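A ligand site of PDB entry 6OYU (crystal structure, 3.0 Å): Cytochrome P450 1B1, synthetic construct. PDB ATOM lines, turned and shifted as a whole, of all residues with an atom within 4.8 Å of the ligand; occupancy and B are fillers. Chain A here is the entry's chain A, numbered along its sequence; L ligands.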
ATOM      1  N   ARG A  79     -11.432 -23.340 -28.046  1.00  0.00           N
ATOM      2  CA  ARG A  79     -10.605 -24.363 -28.657  1.00  0.00           C
ATOM      3  C   ARG A  79     -11.184 -24.699 -30.020  1.00  0.00           C
ATOM      4  O   ARG A  79     -12.405 -24.654 -30.207  1.00  0.00           O
ATOM      5  CB  ARG A  79     -10.539 -25.632 -27.802  1.00  0.00           C
ATOM      6  CG  ARG A  79      -9.841 -25.455 -26.458  1.00  0.00           C
ATOM      7  CD  ARG A  79      -8.333 -25.365 -26.605  1.00  0.00           C
ATOM      8  NE  ARG A  79      -7.648 -25.487 -25.324  1.00  0.00           N
ATOM      9  CZ  ARG A  79      -6.464 -24.949 -25.043  1.00  0.00           C
ATOM     10  NH1 ARG A  79      -5.812 -24.243 -25.956  1.00  0.00           N
ATOM     11  NH2 ARG A  79      -5.924 -25.128 -23.845  1.00  0.00           N
ATOM     12  N   LEU A  94     -11.115 -31.716 -20.761  1.00  0.00           N
ATOM     13  CA  LEU A  94     -10.994 -30.318 -20.373  1.00  0.00           C
ATOM     14  C   LEU A  94      -9.963 -29.601 -21.238  1.00  0.00           C
ATOM     15  O   LEU A  94     -10.148 -28.434 -21.607  1.00  0.00           O
ATOM     16  CB  LEU A  94     -10.628 -30.194 -18.890  1.00  0.00           C
ATOM     17  CG  LEU A  94     -10.385 -28.777 -18.370  1.00  0.00           C
ATOM     18  CD1 LEU A  94     -11.703 -28.026 -18.228  1.00  0.00           C
ATOM     19  CD2 LEU A  94      -9.652 -28.814 -17.038  1.00  0.00           C
ATOM     20  N   ALA A  95      -8.868 -30.287 -21.563  1.00  0.00           N
ATOM     21  CA  ALA A  95      -7.792 -29.655 -22.316  1.00  0.00           C
ATOM     22  C   ALA A  95      -8.248 -29.223 -23.699  1.00  0.00           C
ATOM     23  O   ALA A  95      -7.742 -28.221 -24.234  1.00  0.00           O
ATOM     24  CB  ALA A  95      -6.596 -30.596 -22.420  1.00  0.00           C
ATOM     25  N   TRP A 103     -18.231 -26.241 -19.414  1.00  0.00           N
ATOM     26  CA  TRP A 103     -16.778 -26.352 -19.332  1.00  0.00           C
ATOM     27  C   TRP A 103     -16.236 -25.468 -18.210  1.00  0.00           C
ATOM     28  O   TRP A 103     -15.308 -25.872 -17.491  1.00  0.00           O
ATOM     29  CB  TRP A 103     -16.153 -25.965 -20.670  1.00  0.00           C
ATOM     30  CG  TRP A 103     -14.663 -26.046 -20.694  1.00  0.00           C
ATOM     31  CD1 TRP A 103     -13.910 -27.077 -21.171  1.00  0.00           C
ATOM     32  CD2 TRP A 103     -13.740 -25.067 -20.205  1.00  0.00           C
ATOM     33  NE1 TRP A 103     -12.569 -26.796 -21.021  1.00  0.00           N
ATOM     34  CE2 TRP A 103     -12.436 -25.569 -20.427  1.00  0.00           C
ATOM     35  CE3 TRP A 103     -13.874 -23.803 -19.614  1.00  0.00           C
ATOM     36  CZ2 TRP A 103     -11.293 -24.861 -20.069  1.00  0.00           C
ATOM     37  CZ3 TRP A 103     -12.739 -23.107 -19.265  1.00  0.00           C
ATOM     38  CH2 TRP A 103     -11.463 -23.632 -19.497  1.00  0.00           C
ATOM     39  N   ARG A 107     -13.631 -26.870 -15.448  1.00  0.00           N
ATOM     40  CA  ARG A 107     -12.355 -26.224 -15.168  1.00  0.00           C
ATOM     41  C   ARG A 107     -12.255 -25.806 -13.701  1.00  0.00           C
ATOM     42  O   ARG A 107     -11.253 -26.075 -13.038  1.00  0.00           O
ATOM     43  CB  ARG A 107     -12.179 -25.009 -16.085  1.00  0.00           C
ATOM     44  CG  ARG A 107     -11.107 -24.025 -15.657  1.00  0.00           C
ATOM     45  CD  ARG A 107      -9.804 -24.277 -16.385  1.00  0.00           C
ATOM     46  NE  ARG A 107      -8.670 -23.681 -15.695  1.00  0.00           N
ATOM     47  CZ  ARG A 107      -7.428 -23.651 -16.180  1.00  0.00           C
ATOM     48  NH1 ARG A 107      -7.166 -24.195 -17.357  1.00  0.00           N
ATOM     49  NH2 ARG A 107      -6.452 -23.082 -15.477  1.00  0.00           N
ATOM     50  N   VAL A 114      -6.975 -30.282  -8.244  1.00  0.00           N
ATOM     51  CA  VAL A 114      -5.607 -30.729  -8.477  1.00  0.00           C
ATOM     52  C   VAL A 114      -4.610 -29.838  -7.738  1.00  0.00           C
ATOM     53  O   VAL A 114      -3.527 -30.309  -7.358  1.00  0.00           O
ATOM     54  CB  VAL A 114      -5.287 -30.778  -9.984  1.00  0.00           C
ATOM     55  CG1 VAL A 114      -5.430 -29.418 -10.616  1.00  0.00           C
ATOM     56  CG2 VAL A 114      -3.888 -31.319 -10.213  1.00  0.00           C
ATOM     57  N   MET A 167       2.385 -40.331 -11.464  1.00  0.00           N
ATOM     58  CA  MET A 167       1.017 -39.927 -11.776  1.00  0.00           C
ATOM     59  C   MET A 167       0.066 -41.114 -11.725  1.00  0.00           C
ATOM     60  O   MET A 167      -1.144 -40.930 -11.501  1.00  0.00           O
ATOM     61  CB  MET A 167       0.947 -39.265 -13.145  1.00  0.00           C
ATOM     62  CG  MET A 167       1.942 -38.140 -13.327  1.00  0.00           C
ATOM     63  SD  MET A 167       1.757 -36.778 -12.155  1.00  0.00           S
ATOM     64  CE  MET A 167       0.001 -36.426 -12.225  1.00  0.00           C
ATOM     65  N   MET A 254      -6.266 -38.799  -6.524  1.00  0.00           N
ATOM     66  CA  MET A 254      -6.952 -37.654  -7.118  1.00  0.00           C
ATOM     67  C   MET A 254      -8.307 -38.010  -7.712  1.00  0.00           C
ATOM     68  O   MET A 254      -9.130 -37.108  -7.911  1.00  0.00           O
ATOM     69  CB  MET A 254      -6.074 -37.010  -8.193  1.00  0.00           C
ATOM     70  CG  MET A 254      -5.924 -35.516  -8.009  1.00  0.00           C
ATOM     71  SD  MET A 254      -5.268 -34.723  -9.485  1.00  0.00           S
ATOM     72  CE  MET A 254      -3.528 -34.672  -9.069  1.00  0.00           C
ATOM     73  N   ASP A 288      -7.350 -36.510 -18.762  1.00  0.00           N
ATOM     74  CA  ASP A 288      -6.587 -35.320 -19.097  1.00  0.00           C
ATOM     75  C   ASP A 288      -5.439 -35.132 -18.117  1.00  0.00           C
ATOM     76  O   ASP A 288      -4.291 -34.893 -18.518  1.00  0.00           O
ATOM     77  CB  ASP A 288      -7.497 -34.088 -19.075  1.00  0.00           C
ATOM     78  CG  ASP A 288      -8.221 -33.873 -20.406  1.00  0.00           C
ATOM     79  OD1 ASP A 288      -8.212 -34.777 -21.256  1.00  0.00           O
ATOM     80  OD2 ASP A 288      -8.794 -32.782 -20.580  1.00  0.00           O
ATOM     81  N   ILE A 289      -5.726 -35.249 -16.820  1.00  0.00           N
ATOM     82  CA  ILE A 289      -4.713 -35.007 -15.794  1.00  0.00           C
ATOM     83  C   ILE A 289      -3.513 -35.935 -15.998  1.00  0.00           C
ATOM     84  O   ILE A 289      -2.361 -35.500 -16.005  1.00  0.00           O
ATOM     85  CB  ILE A 289      -5.324 -35.158 -14.395  1.00  0.00           C
ATOM     86  CG1 ILE A 289      -6.093 -33.887 -14.028  1.00  0.00           C
ATOM     87  CG2 ILE A 289      -4.250 -35.447 -13.353  1.00  0.00           C
ATOM     88  CD1 ILE A 289      -7.003 -34.027 -12.836  1.00  0.00           C
ATOM     89  N   ALA A 292      -1.797 -35.017 -19.946  1.00  0.00           N
ATOM     90  CA  ALA A 292      -0.966 -33.818 -20.051  1.00  0.00           C
ATOM     91  C   ALA A 292       0.252 -33.882 -19.138  1.00  0.00           C
ATOM     92  O   ALA A 292       1.159 -33.057 -19.294  1.00  0.00           O
ATOM     93  CB  ALA A 292      -1.787 -32.575 -19.721  1.00  0.00           C
ATOM     94  N   SER A 293       0.289 -34.838 -18.215  1.00  0.00           N
ATOM     95  CA  SER A 293       1.368 -34.938 -17.239  1.00  0.00           C
ATOM     96  C   SER A 293       2.604 -35.659 -17.766  1.00  0.00           C
ATOM     97  O   SER A 293       3.693 -35.454 -17.214  1.00  0.00           O
ATOM     98  CB  SER A 293       0.844 -35.696 -16.010  1.00  0.00           C
ATOM     99  OG  SER A 293       1.848 -35.788 -15.024  1.00  0.00           O
ATOM    100  N   THR A 296       5.316 -33.794 -20.638  1.00  0.00           N
ATOM    101  CA  THR A 296       5.783 -32.523 -20.103  1.00  0.00           C
ATOM    102  C   THR A 296       6.770 -32.724 -18.959  1.00  0.00           C
ATOM    103  O   THR A 296       7.884 -32.198 -18.983  1.00  0.00           O
ATOM    104  CB  THR A 296       4.596 -31.672 -19.658  1.00  0.00           C
ATOM    105  OG1 THR A 296       3.763 -32.434 -18.762  1.00  0.00           O
ATOM    106  CG2 THR A 296       3.775 -31.235 -20.855  1.00  0.00           C
ATOM    107  N   LEU A 297       6.370 -33.500 -17.941  1.00  0.00           N
ATOM    108  CA  LEU A 297       7.265 -33.728 -16.800  1.00  0.00           C
ATOM    109  C   LEU A 297       8.483 -34.548 -17.204  1.00  0.00           C
ATOM    110  O   LEU A 297       9.589 -34.294 -16.728  1.00  0.00           O
ATOM    111  CB  LEU A 297       6.497 -34.405 -15.667  1.00  0.00           C
ATOM    112  CG  LEU A 297       5.397 -33.555 -15.028  1.00  0.00           C
ATOM    113  CD1 LEU A 297       4.620 -34.340 -13.982  1.00  0.00           C
ATOM    114  CD2 LEU A 297       5.977 -32.287 -14.411  1.00  0.00           C
ATOM    115  N   ALA A 300      10.894 -32.146 -18.789  1.00  0.00           N
ATOM    116  CA  ALA A 300      11.491 -31.254 -17.806  1.00  0.00           C
ATOM    117  C   ALA A 300      12.657 -31.933 -17.084  1.00  0.00           C
ATOM    118  O   ALA A 300      13.747 -31.354 -16.968  1.00  0.00           O
ATOM    119  CB  ALA A 300      10.437 -30.792 -16.801  1.00  0.00           C
ATOM    120  N   PHE A 356      10.362 -25.863 -23.254  1.00  0.00           N
ATOM    121  CA  PHE A 356      10.094 -27.107 -23.973  1.00  0.00           C
ATOM    122  C   PHE A 356       8.647 -27.254 -24.405  1.00  0.00           C
ATOM    123  O   PHE A 356       8.340 -28.158 -25.183  1.00  0.00           O
ATOM    124  CB  PHE A 356      10.522 -28.317 -23.122  1.00  0.00           C
ATOM    125  CG  PHE A 356       9.954 -28.328 -21.733  1.00  0.00           C
ATOM    126  CD1 PHE A 356       8.693 -28.845 -21.491  1.00  0.00           C
ATOM    127  CD2 PHE A 356      10.688 -27.838 -20.669  1.00  0.00           C
ATOM    128  CE1 PHE A 356       8.171 -28.867 -20.206  1.00  0.00           C
ATOM    129  CE2 PHE A 356      10.176 -27.851 -19.385  1.00  0.00           C
ATOM    130  CZ  PHE A 356       8.918 -28.371 -19.152  1.00  0.00           C
ATOM    131  N   VAL A 357       7.750 -26.390 -23.924  1.00  0.00           N
ATOM    132  CA  VAL A 357       6.411 -26.255 -24.512  1.00  0.00           C
ATOM    133  C   VAL A 357       6.401 -24.928 -25.263  1.00  0.00           C
ATOM    134  O   VAL A 357       5.823 -23.939 -24.784  1.00  0.00           O
ATOM    135  CB  VAL A 357       5.315 -26.305 -23.448  1.00  0.00           C
ATOM    136  CG1 VAL A 357       3.942 -26.479 -24.100  1.00  0.00           C
ATOM    137  CG2 VAL A 357       5.576 -27.446 -22.466  1.00  0.00           C
ATOM    138  N   THR A 360       1.547 -23.379 -26.929  1.00  0.00           N
ATOM    139  CA  THR A 360       0.498 -23.964 -26.120  1.00  0.00           C
ATOM    140  C   THR A 360      -0.456 -24.770 -26.992  1.00  0.00           C
ATOM    141  O   THR A 360      -0.308 -24.843 -28.222  1.00  0.00           O
ATOM    142  CB  THR A 360      -0.273 -22.882 -25.362  1.00  0.00           C
ATOM    143  OG1 THR A 360      -1.179 -22.219 -26.262  1.00  0.00           O
ATOM    144  CG2 THR A 360       0.659 -21.856 -24.745  1.00  0.00           C
ATOM    145  N   ILE A 361      -1.442 -25.400 -26.357  1.00  0.00           N
ATOM    146  CA  ILE A 361      -2.508 -26.050 -27.111  1.00  0.00           C
ATOM    147  C   ILE A 361      -3.239 -24.991 -27.938  1.00  0.00           C
ATOM    148  O   ILE A 361      -3.574 -23.918 -27.402  1.00  0.00           O
ATOM    149  CB  ILE A 361      -3.476 -26.781 -26.172  1.00  0.00           C
ATOM    150  CG1 ILE A 361      -2.783 -27.971 -25.519  1.00  0.00           C
ATOM    151  CG2 ILE A 361      -4.711 -27.250 -26.915  1.00  0.00           C
ATOM    152  CD1 ILE A 361      -3.452 -28.448 -24.250  1.00  0.00           C
ATOM    153  N   HIS A 363      -5.482 -22.279 -29.407  1.00  0.00           N
ATOM    154  CA  HIS A 363      -6.640 -21.549 -28.907  1.00  0.00           C
ATOM    155  C   HIS A 363      -7.632 -21.269 -30.033  1.00  0.00           C
ATOM    156  O   HIS A 363      -7.349 -21.484 -31.219  1.00  0.00           O
ATOM    157  CB  HIS A 363      -6.200 -20.234 -28.264  1.00  0.00           C
ATOM    158  CG  HIS A 363      -5.538 -20.402 -26.931  1.00  0.00           C
ATOM    159  ND1 HIS A 363      -6.132 -20.021 -25.744  1.00  0.00           N
ATOM    160  CD2 HIS A 363      -4.319 -20.894 -26.596  1.00  0.00           C
ATOM    161  CE1 HIS A 363      -5.316 -20.284 -24.741  1.00  0.00           C
ATOM    162  NE2 HIS A 363      -4.214 -20.819 -25.228  1.00  0.00           N
ATOM    163  N   GLN A 386       5.051 -19.194 -26.723  1.00  0.00           N
ATOM    164  CA  GLN A 386       5.658 -18.881 -25.433  1.00  0.00           C
ATOM    165  C   GLN A 386       7.164 -18.664 -25.576  1.00  0.00           C
ATOM    166  O   GLN A 386       7.749 -17.833 -24.879  1.00  0.00           O
ATOM    167  CB  GLN A 386       5.392 -20.008 -24.446  1.00  0.00           C
ATOM    168  CG  GLN A 386       3.927 -20.339 -24.257  1.00  0.00           C
ATOM    169  CD  GLN A 386       3.702 -21.425 -23.230  1.00  0.00           C
ATOM    170  OE1 GLN A 386       3.233 -21.169 -22.124  1.00  0.00           O
ATOM    171  NE2 GLN A 386       4.029 -22.659 -23.600  1.00  0.00           N
ATOM    172  N   ILE A 424       5.917 -20.806 -19.441  1.00  0.00           N
ATOM    173  CA  ILE A 424       5.990 -22.185 -19.905  1.00  0.00           C
ATOM    174  C   ILE A 424       4.629 -22.870 -19.797  1.00  0.00           C
ATOM    175  O   ILE A 424       4.227 -23.614 -20.691  1.00  0.00           O
ATOM    176  CB  ILE A 424       7.082 -22.959 -19.130  1.00  0.00           C
ATOM    177  CG1 ILE A 424       7.179 -24.408 -19.609  1.00  0.00           C
ATOM    178  CG2 ILE A 424       6.818 -22.918 -17.639  1.00  0.00           C
ATOM    179  CD1 ILE A 424       8.084 -24.584 -20.814  1.00  0.00           C
ATOM    180  N   PHE A 425       3.923 -22.631 -18.692  1.00  0.00           N
ATOM    181  CA  PHE A 425       2.473 -22.747 -18.694  1.00  0.00           C
ATOM    182  C   PHE A 425       1.900 -21.454 -19.252  1.00  0.00           C
ATOM    183  O   PHE A 425       2.517 -20.391 -19.154  1.00  0.00           O
ATOM    184  CB  PHE A 425       1.951 -22.993 -17.277  1.00  0.00           C
ATOM    185  CG  PHE A 425       2.725 -24.018 -16.503  1.00  0.00           C
ATOM    186  CD1 PHE A 425       2.407 -25.358 -16.593  1.00  0.00           C
ATOM    187  CD2 PHE A 425       3.777 -23.639 -15.681  1.00  0.00           C
ATOM    188  CE1 PHE A 425       3.114 -26.303 -15.882  1.00  0.00           C
ATOM    189  CE2 PHE A 425       4.504 -24.574 -14.968  1.00  0.00           C
ATOM    190  CZ  PHE A 425       4.168 -25.918 -15.072  1.00  0.00           C
ATOM    191  N   SER A 426       0.717 -21.548 -19.839  1.00  0.00           N
ATOM    192  CA  SER A 426       0.146 -20.362 -20.482  1.00  0.00           C
ATOM    193  C   SER A 426      -0.389 -19.406 -19.423  1.00  0.00           C
ATOM    194  O   SER A 426      -0.020 -19.486 -18.244  1.00  0.00           O
ATOM    195  CB  SER A 426      -0.960 -20.772 -21.459  1.00  0.00           C
ATOM    196  OG  SER A 426      -1.225 -19.728 -22.380  1.00  0.00           O
ATOM    197  N   VAL A 427      -1.253 -18.479 -19.834  1.00  0.00           N
ATOM    198  CA  VAL A 427      -1.969 -17.604 -18.914  1.00  0.00           C
ATOM    199  C   VAL A 427      -3.381 -17.422 -19.460  1.00  0.00           C
ATOM    200  O   VAL A 427      -3.715 -17.864 -20.558  1.00  0.00           O
ATOM    201  CB  VAL A 427      -1.269 -16.253 -18.701  1.00  0.00           C
ATOM    202  CG1 VAL A 427       0.161 -16.468 -18.227  1.00  0.00           C
ATOM    203  CG2 VAL A 427      -1.290 -15.422 -19.981  1.00  0.00           C
ATOM    204  N   LYS A 429      -7.614 -17.935 -19.108  1.00  0.00           N
ATOM    205  CA  LYS A 429      -8.556 -18.927 -18.598  1.00  0.00           C
ATOM    206  C   LYS A 429      -8.165 -20.363 -18.934  1.00  0.00           C
ATOM    207  O   LYS A 429      -8.766 -21.294 -18.391  1.00  0.00           O
ATOM    208  CB  LYS A 429      -9.955 -18.646 -19.160  1.00  0.00           C
ATOM    209  CG  LYS A 429     -10.420 -17.209 -18.983  1.00  0.00           C
ATOM    210  CD  LYS A 429     -11.741 -17.123 -18.220  1.00  0.00           C
ATOM    211  CE  LYS A 429     -11.992 -15.716 -17.701  1.00  0.00           C
ATOM    212  NZ  LYS A 429     -12.212 -15.702 -16.223  1.00  0.00           N
ATOM    213  N   ARG A 430      -7.166 -20.565 -19.807  1.00  0.00           N
ATOM    214  CA  ARG A 430      -6.732 -21.904 -20.193  1.00  0.00           C
ATOM    215  C   ARG A 430      -5.350 -22.251 -19.647  1.00  0.00           C
ATOM    216  O   ARG A 430      -4.794 -23.285 -20.033  1.00  0.00           O
ATOM    217  CB  ARG A 430      -6.749 -22.049 -21.711  1.00  0.00           C
ATOM    218  CG  ARG A 430      -8.124 -21.951 -22.362  1.00  0.00           C
ATOM    219  CD  ARG A 430      -9.170 -22.759 -21.601  1.00  0.00           C
ATOM    220  NE  ARG A 430     -10.209 -23.289 -22.471  1.00  0.00           N
ATOM    221  CZ  ARG A 430     -10.207 -24.513 -22.989  1.00  0.00           C
ATOM    222  NH1 ARG A 430      -9.220 -25.350 -22.747  1.00  0.00           N
ATOM    223  NH2 ARG A 430     -11.218 -24.902 -23.766  1.00  0.00           N
ATOM    224  N   ARG A 431      -4.791 -21.426 -18.761  1.00  0.00           N
ATOM    225  CA  ARG A 431      -3.504 -21.733 -18.166  1.00  0.00           C
ATOM    226  C   ARG A 431      -3.518 -23.110 -17.523  1.00  0.00           C
ATOM    227  O   ARG A 431      -4.535 -23.545 -16.977  1.00  0.00           O
ATOM    228  CB  ARG A 431      -3.140 -20.672 -17.120  1.00  0.00           C
ATOM    229  CG  ARG A 431      -4.072 -20.644 -15.931  1.00  0.00           C
ATOM    230  CD  ARG A 431      -3.878 -19.399 -15.080  1.00  0.00           C
ATOM    231  NE  ARG A 431      -4.699 -19.436 -13.876  1.00  0.00           N
ATOM    232  CZ  ARG A 431      -6.008 -19.185 -13.837  1.00  0.00           C
ATOM    233  NH1 ARG A 431      -6.654 -18.859 -14.945  1.00  0.00           N
ATOM    234  NH2 ARG A 431      -6.660 -19.249 -12.690  1.00  0.00           N
ATOM    235  N   CYS A 432      -2.392 -23.810 -17.600  1.00  0.00           N
ATOM    236  CA  CYS A 432      -2.287 -25.154 -17.068  1.00  0.00           C
ATOM    237  C   CYS A 432      -2.803 -25.219 -15.639  1.00  0.00           C
ATOM    238  O   CYS A 432      -2.413 -24.411 -14.779  1.00  0.00           O
ATOM    239  CB  CYS A 432      -0.830 -25.605 -17.117  1.00  0.00           C
ATOM    240  SG  CYS A 432      -0.474 -27.088 -16.178  1.00  0.00           S
ATOM    241  N   ILE A 433      -3.666 -26.212 -15.368  1.00  0.00           N
ATOM    242  CA  ILE A 433      -4.192 -26.414 -14.019  1.00  0.00           C
ATOM    243  C   ILE A 433      -3.229 -27.180 -13.138  1.00  0.00           C
ATOM    244  O   ILE A 433      -3.521 -27.390 -11.943  1.00  0.00           O
ATOM    245  CB  ILE A 433      -5.536 -27.162 -14.017  1.00  0.00           C
ATOM    246  CG1 ILE A 433      -5.398 -28.555 -14.622  1.00  0.00           C
ATOM    247  CG2 ILE A 433      -6.586 -26.381 -14.795  1.00  0.00           C
ATOM    248  CD1 ILE A 433      -6.535 -29.489 -14.243  1.00  0.00           C
ATOM    249  N   GLY A 434      -2.105 -27.637 -13.676  1.00  0.00           N
ATOM    250  CA  GLY A 434      -1.127 -28.371 -12.898  1.00  0.00           C
ATOM    251  C   GLY A 434       0.171 -27.610 -12.754  1.00  0.00           C
ATOM    252  O   GLY A 434       1.223 -28.207 -12.494  1.00  0.00           O
ATOM    253  N   LEU A 437       1.366 -27.981  -9.228  1.00  0.00           N
ATOM    254  CA  LEU A 437       1.607 -29.386  -8.912  1.00  0.00           C
ATOM    255  C   LEU A 437       2.907 -29.879  -9.535  1.00  0.00           C
ATOM    256  O   LEU A 437       3.566 -30.757  -8.964  1.00  0.00           O
ATOM    257  CB  LEU A 437       0.432 -30.240  -9.384  1.00  0.00           C
ATOM    258  CG  LEU A 437       0.534 -31.735  -9.085  1.00  0.00           C
ATOM    259  CD1 LEU A 437      -0.350 -32.111  -7.911  1.00  0.00           C
ATOM    260  CD2 LEU A 437       0.150 -32.544 -10.309  1.00  0.00           C
ATOM    261  N   SER A 438       3.280 -29.340 -10.692  1.00  0.00           N
ATOM    262  CA  SER A 438       4.476 -29.797 -11.395  1.00  0.00           C
ATOM    263  C   SER A 438       5.742 -29.123 -10.910  1.00  0.00           C
ATOM    264  O   SER A 438       6.806 -29.751 -10.863  1.00  0.00           O
ATOM    265  CB  SER A 438       4.309 -29.575 -12.901  1.00  0.00           C
ATOM    266  OG  SER A 438       3.590 -28.382 -13.153  1.00  0.00           O
ATOM    267  N   LEU A 442       8.450 -31.321  -9.546  1.00  0.00           N
ATOM    268  CA  LEU A 442       9.785 -31.208 -10.120  1.00  0.00           C
ATOM    269  C   LEU A 442      10.804 -30.856  -9.040  1.00  0.00           C
ATOM    270  O   LEU A 442      11.882 -31.447  -8.968  1.00  0.00           O
ATOM    271  CB  LEU A 442       9.794 -30.154 -11.234  1.00  0.00           C
ATOM    272  CG  LEU A 442       9.140 -30.603 -12.538  1.00  0.00           C
ATOM    273  CD1 LEU A 442       8.816 -29.412 -13.433  1.00  0.00           C
ATOM    274  CD2 LEU A 442      10.035 -31.599 -13.259  1.00  0.00           C
HETATM  275  C1  LIG L   1      -2.804 -27.203 -20.267  1.00  0.00           C
HETATM  276  C2  LIG L   1       2.016 -26.954 -19.856  1.00  0.00           C
HETATM  277  C3  LIG L   1       1.921 -30.554 -16.601  1.00  0.00           C
HETATM  278  C4  LIG L   1      -2.909 -30.459 -16.690  1.00  0.00           C
HETATM  279  C5  LIG L   1      -1.483 -26.863 -20.495  1.00  0.00           C
HETATM  280  C6  LIG L   1      -1.001 -25.969 -21.518  1.00  0.00           C
HETATM  281  C7  LIG L   1       0.329 -25.896 -21.403  1.00  0.00           C
HETATM  282  C8  LIG L   1       0.734 -26.741 -20.304  1.00  0.00           C
HETATM  283  C9  LIG L   1       1.272 -25.054 -22.286  1.00  0.00           C
HETATM  284  C10 LIG L   1      -1.863 -25.234 -22.558  1.00  0.00           C
HETATM  285  C11 LIG L   1      -2.360 -23.905 -22.001  1.00  0.00           C
HETATM  286  C12 LIG L   1      -3.010 -23.108 -23.104  1.00  0.00           C
HETATM  287  O1  LIG L   1      -3.116 -21.861 -22.962  1.00  0.00           O
HETATM  288  O2  LIG L   1      -3.421 -23.714 -24.138  1.00  0.00           O
HETATM  289  C13 LIG L   1       2.409 -27.886 -18.916  1.00  0.00           C
HETATM  290  C14 LIG L   1       3.766 -28.096 -18.440  1.00  0.00           C
HETATM  291  C15 LIG L   1       3.738 -29.096 -17.540  1.00  0.00           C
HETATM  292  C16 LIG L   1       2.372 -29.547 -17.419  1.00  0.00           C
HETATM  293  C17 LIG L   1       4.970 -27.269 -18.920  1.00  0.00           C
HETATM  294  C18 LIG L   1       4.901 -29.696 -16.725  1.00  0.00           C
HETATM  295  C19 LIG L   1       6.118 -29.144 -16.709  1.00  0.00           C
HETATM  296  C20 LIG L   1       0.607 -30.784 -16.277  1.00  0.00           C
HETATM  297  C21 LIG L   1       0.113 -31.579 -15.169  1.00  0.00           C
HETATM  298  C22 LIG L   1      -1.226 -31.556 -15.207  1.00  0.00           C
HETATM  299  C23 LIG L   1      -1.615 -30.729 -16.329  1.00  0.00           C
HETATM  300  C24 LIG L   1       1.013 -32.334 -14.156  1.00  0.00           C
HETATM  301  C25 LIG L   1      -2.255 -32.221 -14.271  1.00  0.00           C
HETATM  302  C26 LIG L   1      -1.904 -32.663 -13.050  1.00  0.00           C
HETATM  303  C27 LIG L   1      -3.293 -29.623 -17.706  1.00  0.00           C
HETATM  304  C28 LIG L   1      -4.638 -29.457 -18.187  1.00  0.00           C
HETATM  305  C29 LIG L   1      -4.608 -28.565 -19.172  1.00  0.00           C
HETATM  306  C30 LIG L   1      -3.240 -28.118 -19.345  1.00  0.00           C
HETATM  307  C31 LIG L   1      -5.886 -30.204 -17.657  1.00  0.00           C
HETATM  308  C32 LIG L   1      -5.824 -28.073 -19.978  1.00  0.00           C
HETATM  309  C33 LIG L   1      -6.386 -26.835 -19.281  1.00  0.00           C
HETATM  310  C34 LIG L   1      -7.328 -26.102 -20.200  1.00  0.00           C
HETATM  311  O3  LIG L   1      -8.202 -25.375 -19.683  1.00  0.00           O
HETATM  312  O4  LIG L   1      -7.196 -26.250 -21.444  1.00  0.00           O
HETATM  313  N1  LIG L   1      -0.401 -27.319 -19.775  1.00  0.00           N
HETATM  314  N2  LIG L   1       1.589 -28.785 -18.276  1.00  0.00           N
HETATM  315  N3  LIG L   1      -0.475 -30.275 -16.959  1.00  0.00           N
HETATM  316  N4  LIG L   1      -2.461 -28.790 -18.431  1.00  0.00           N
HETATM  317 FE1  LIG L   1      -0.391 -28.700 -18.310  1.00  0.00          FE
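A ring nitrogen (NE2) of His 363 lies within hydrogen-bond range of an oxygen (O1) of the ligand (2.7 Å).
The guanidinium group (NH2) of Arg 79 is in salt-bridge range of an oxygen (O2) of the ligand.
An oxygen (O4) of the ligand is in salt-bridge range of the guanidinium group of Arg 430, 2.6 Å away.
The side-chain hydroxyl (OG) of Ser 426 lies close to an oxygen (O1) of the ligand (2.9 Å).
O2 of the ligand lies within hydrogen-bond range of OG1 of Thr 360 (3.4 Å).
An oxygen (O3) of the ligand lies within salt-bridge range of the guanidinium group (NH1) of Arg 107.
The side-chain sulfur (SG) of Cys 432 is bound to an iron atom (FE1) of the ligand, 2.7 Å away.
An oxygen (O2) of the ligand sits at hydrogen-bond distance from the backbone NH (N) of Ile 361 (3.4 Å).
The backbone carbonyl oxygen of Ile 361 is in hydrogen-bond range of the guanidinium group of Arg 79.
The side-chain hydroxyl (OG1) of Thr 360 sits close to a ring nitrogen (NE2) of His 363 (3.5 Å).
The guanidinium group of Arg 107 is in hydrogen-bond range of the backbone carbonyl oxygen of Arg 431 (2.5 Å).
The indole nitrogen (NE1) of Trp 103 lies within hydrogen-bond range of the backbone carbonyl oxygen (O) of Leu 94, at 3.0 Å.
The side-chain hydroxyl (OG) of Ser 438 sits at hydrogen-bond distance from the backbone carbonyl oxygen (O) of Gly 434, 2.5 Å away.
The side-chain sulfur (SD) of Met 167 sits close to the side-chain hydroxyl (OG) of Ser 293 (3.0 Å).
The side-chain carboxylate of Asp 288 lies within hydrogen-bond range of the backbone NH of Ala 95 (2.7 Å).
O of Ile 424 sits close to OE1 of Gln 386, 3.0 Å away.
An oxygen (O4) of the ligand lies close to the backbone carbonyl oxygen of Ala 95, at 3.5 Å.
Leu 94 touches the ligand (O to O4, 3.7 Å).
Trp 103 touches the ligand (CZ2 to O3, 3.2 Å).
Val 114 touches the ligand.
Ile 289 touches the ligand (CG2 to C26, 3.7 Å).
Ala 292 touches the ligand (O to C3, 3.8 Å).
OG of Ser 293 touches C24 of the ligand, 3.7 Å away.
Thr 296 touches the ligand (OG1 to C3, 3.4 Å).
CD2 of Leu 297 touches C18 of the ligand (3.6 Å).
CZ of Phe 356 touches C19 of the ligand (3.8 Å).
Val 357 touches the ligand.
Gln 386 touches the ligand.
O of Ile 424 touches C9 of the ligand, 3.7 Å away.
Phe 425 touches the ligand.
CG1 of Ile 433 touches C31 of the ligand (3.5 Å).
Gly 434 touches the ligand.
Leu 437 touches the ligand.
CB of Ser 438 touches C18 of the ligand, 3.9 Å away.
Hydrophobic or aromatic side chains that line the ligand: Ala 95, Trp 103, Val 114, Ile 289, Ala 292, Leu 297, Phe 356, Val 357, Ile 361, His 363, Ile 424, Phe 425, Ile 433 and Leu 437.
26 residues have an atom within 4 Å of the ligand: Arg 79, Leu 94, Ala 95, Trp 103, Arg 107, Val 114, Ile 289, Ala 292, Ser 293, Thr 296, Leu 297, Phe 356, Val 357, Thr 360, Ile 361, His 363, Gln 386, Ile 424, Phe 425, Ser 426, Arg 430, Cys 432, Ile 433, Gly 434, Leu 437 and Ser 438.
The nearest printed residue that does not touch the ligand is Leu 442 (4.3 Å).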
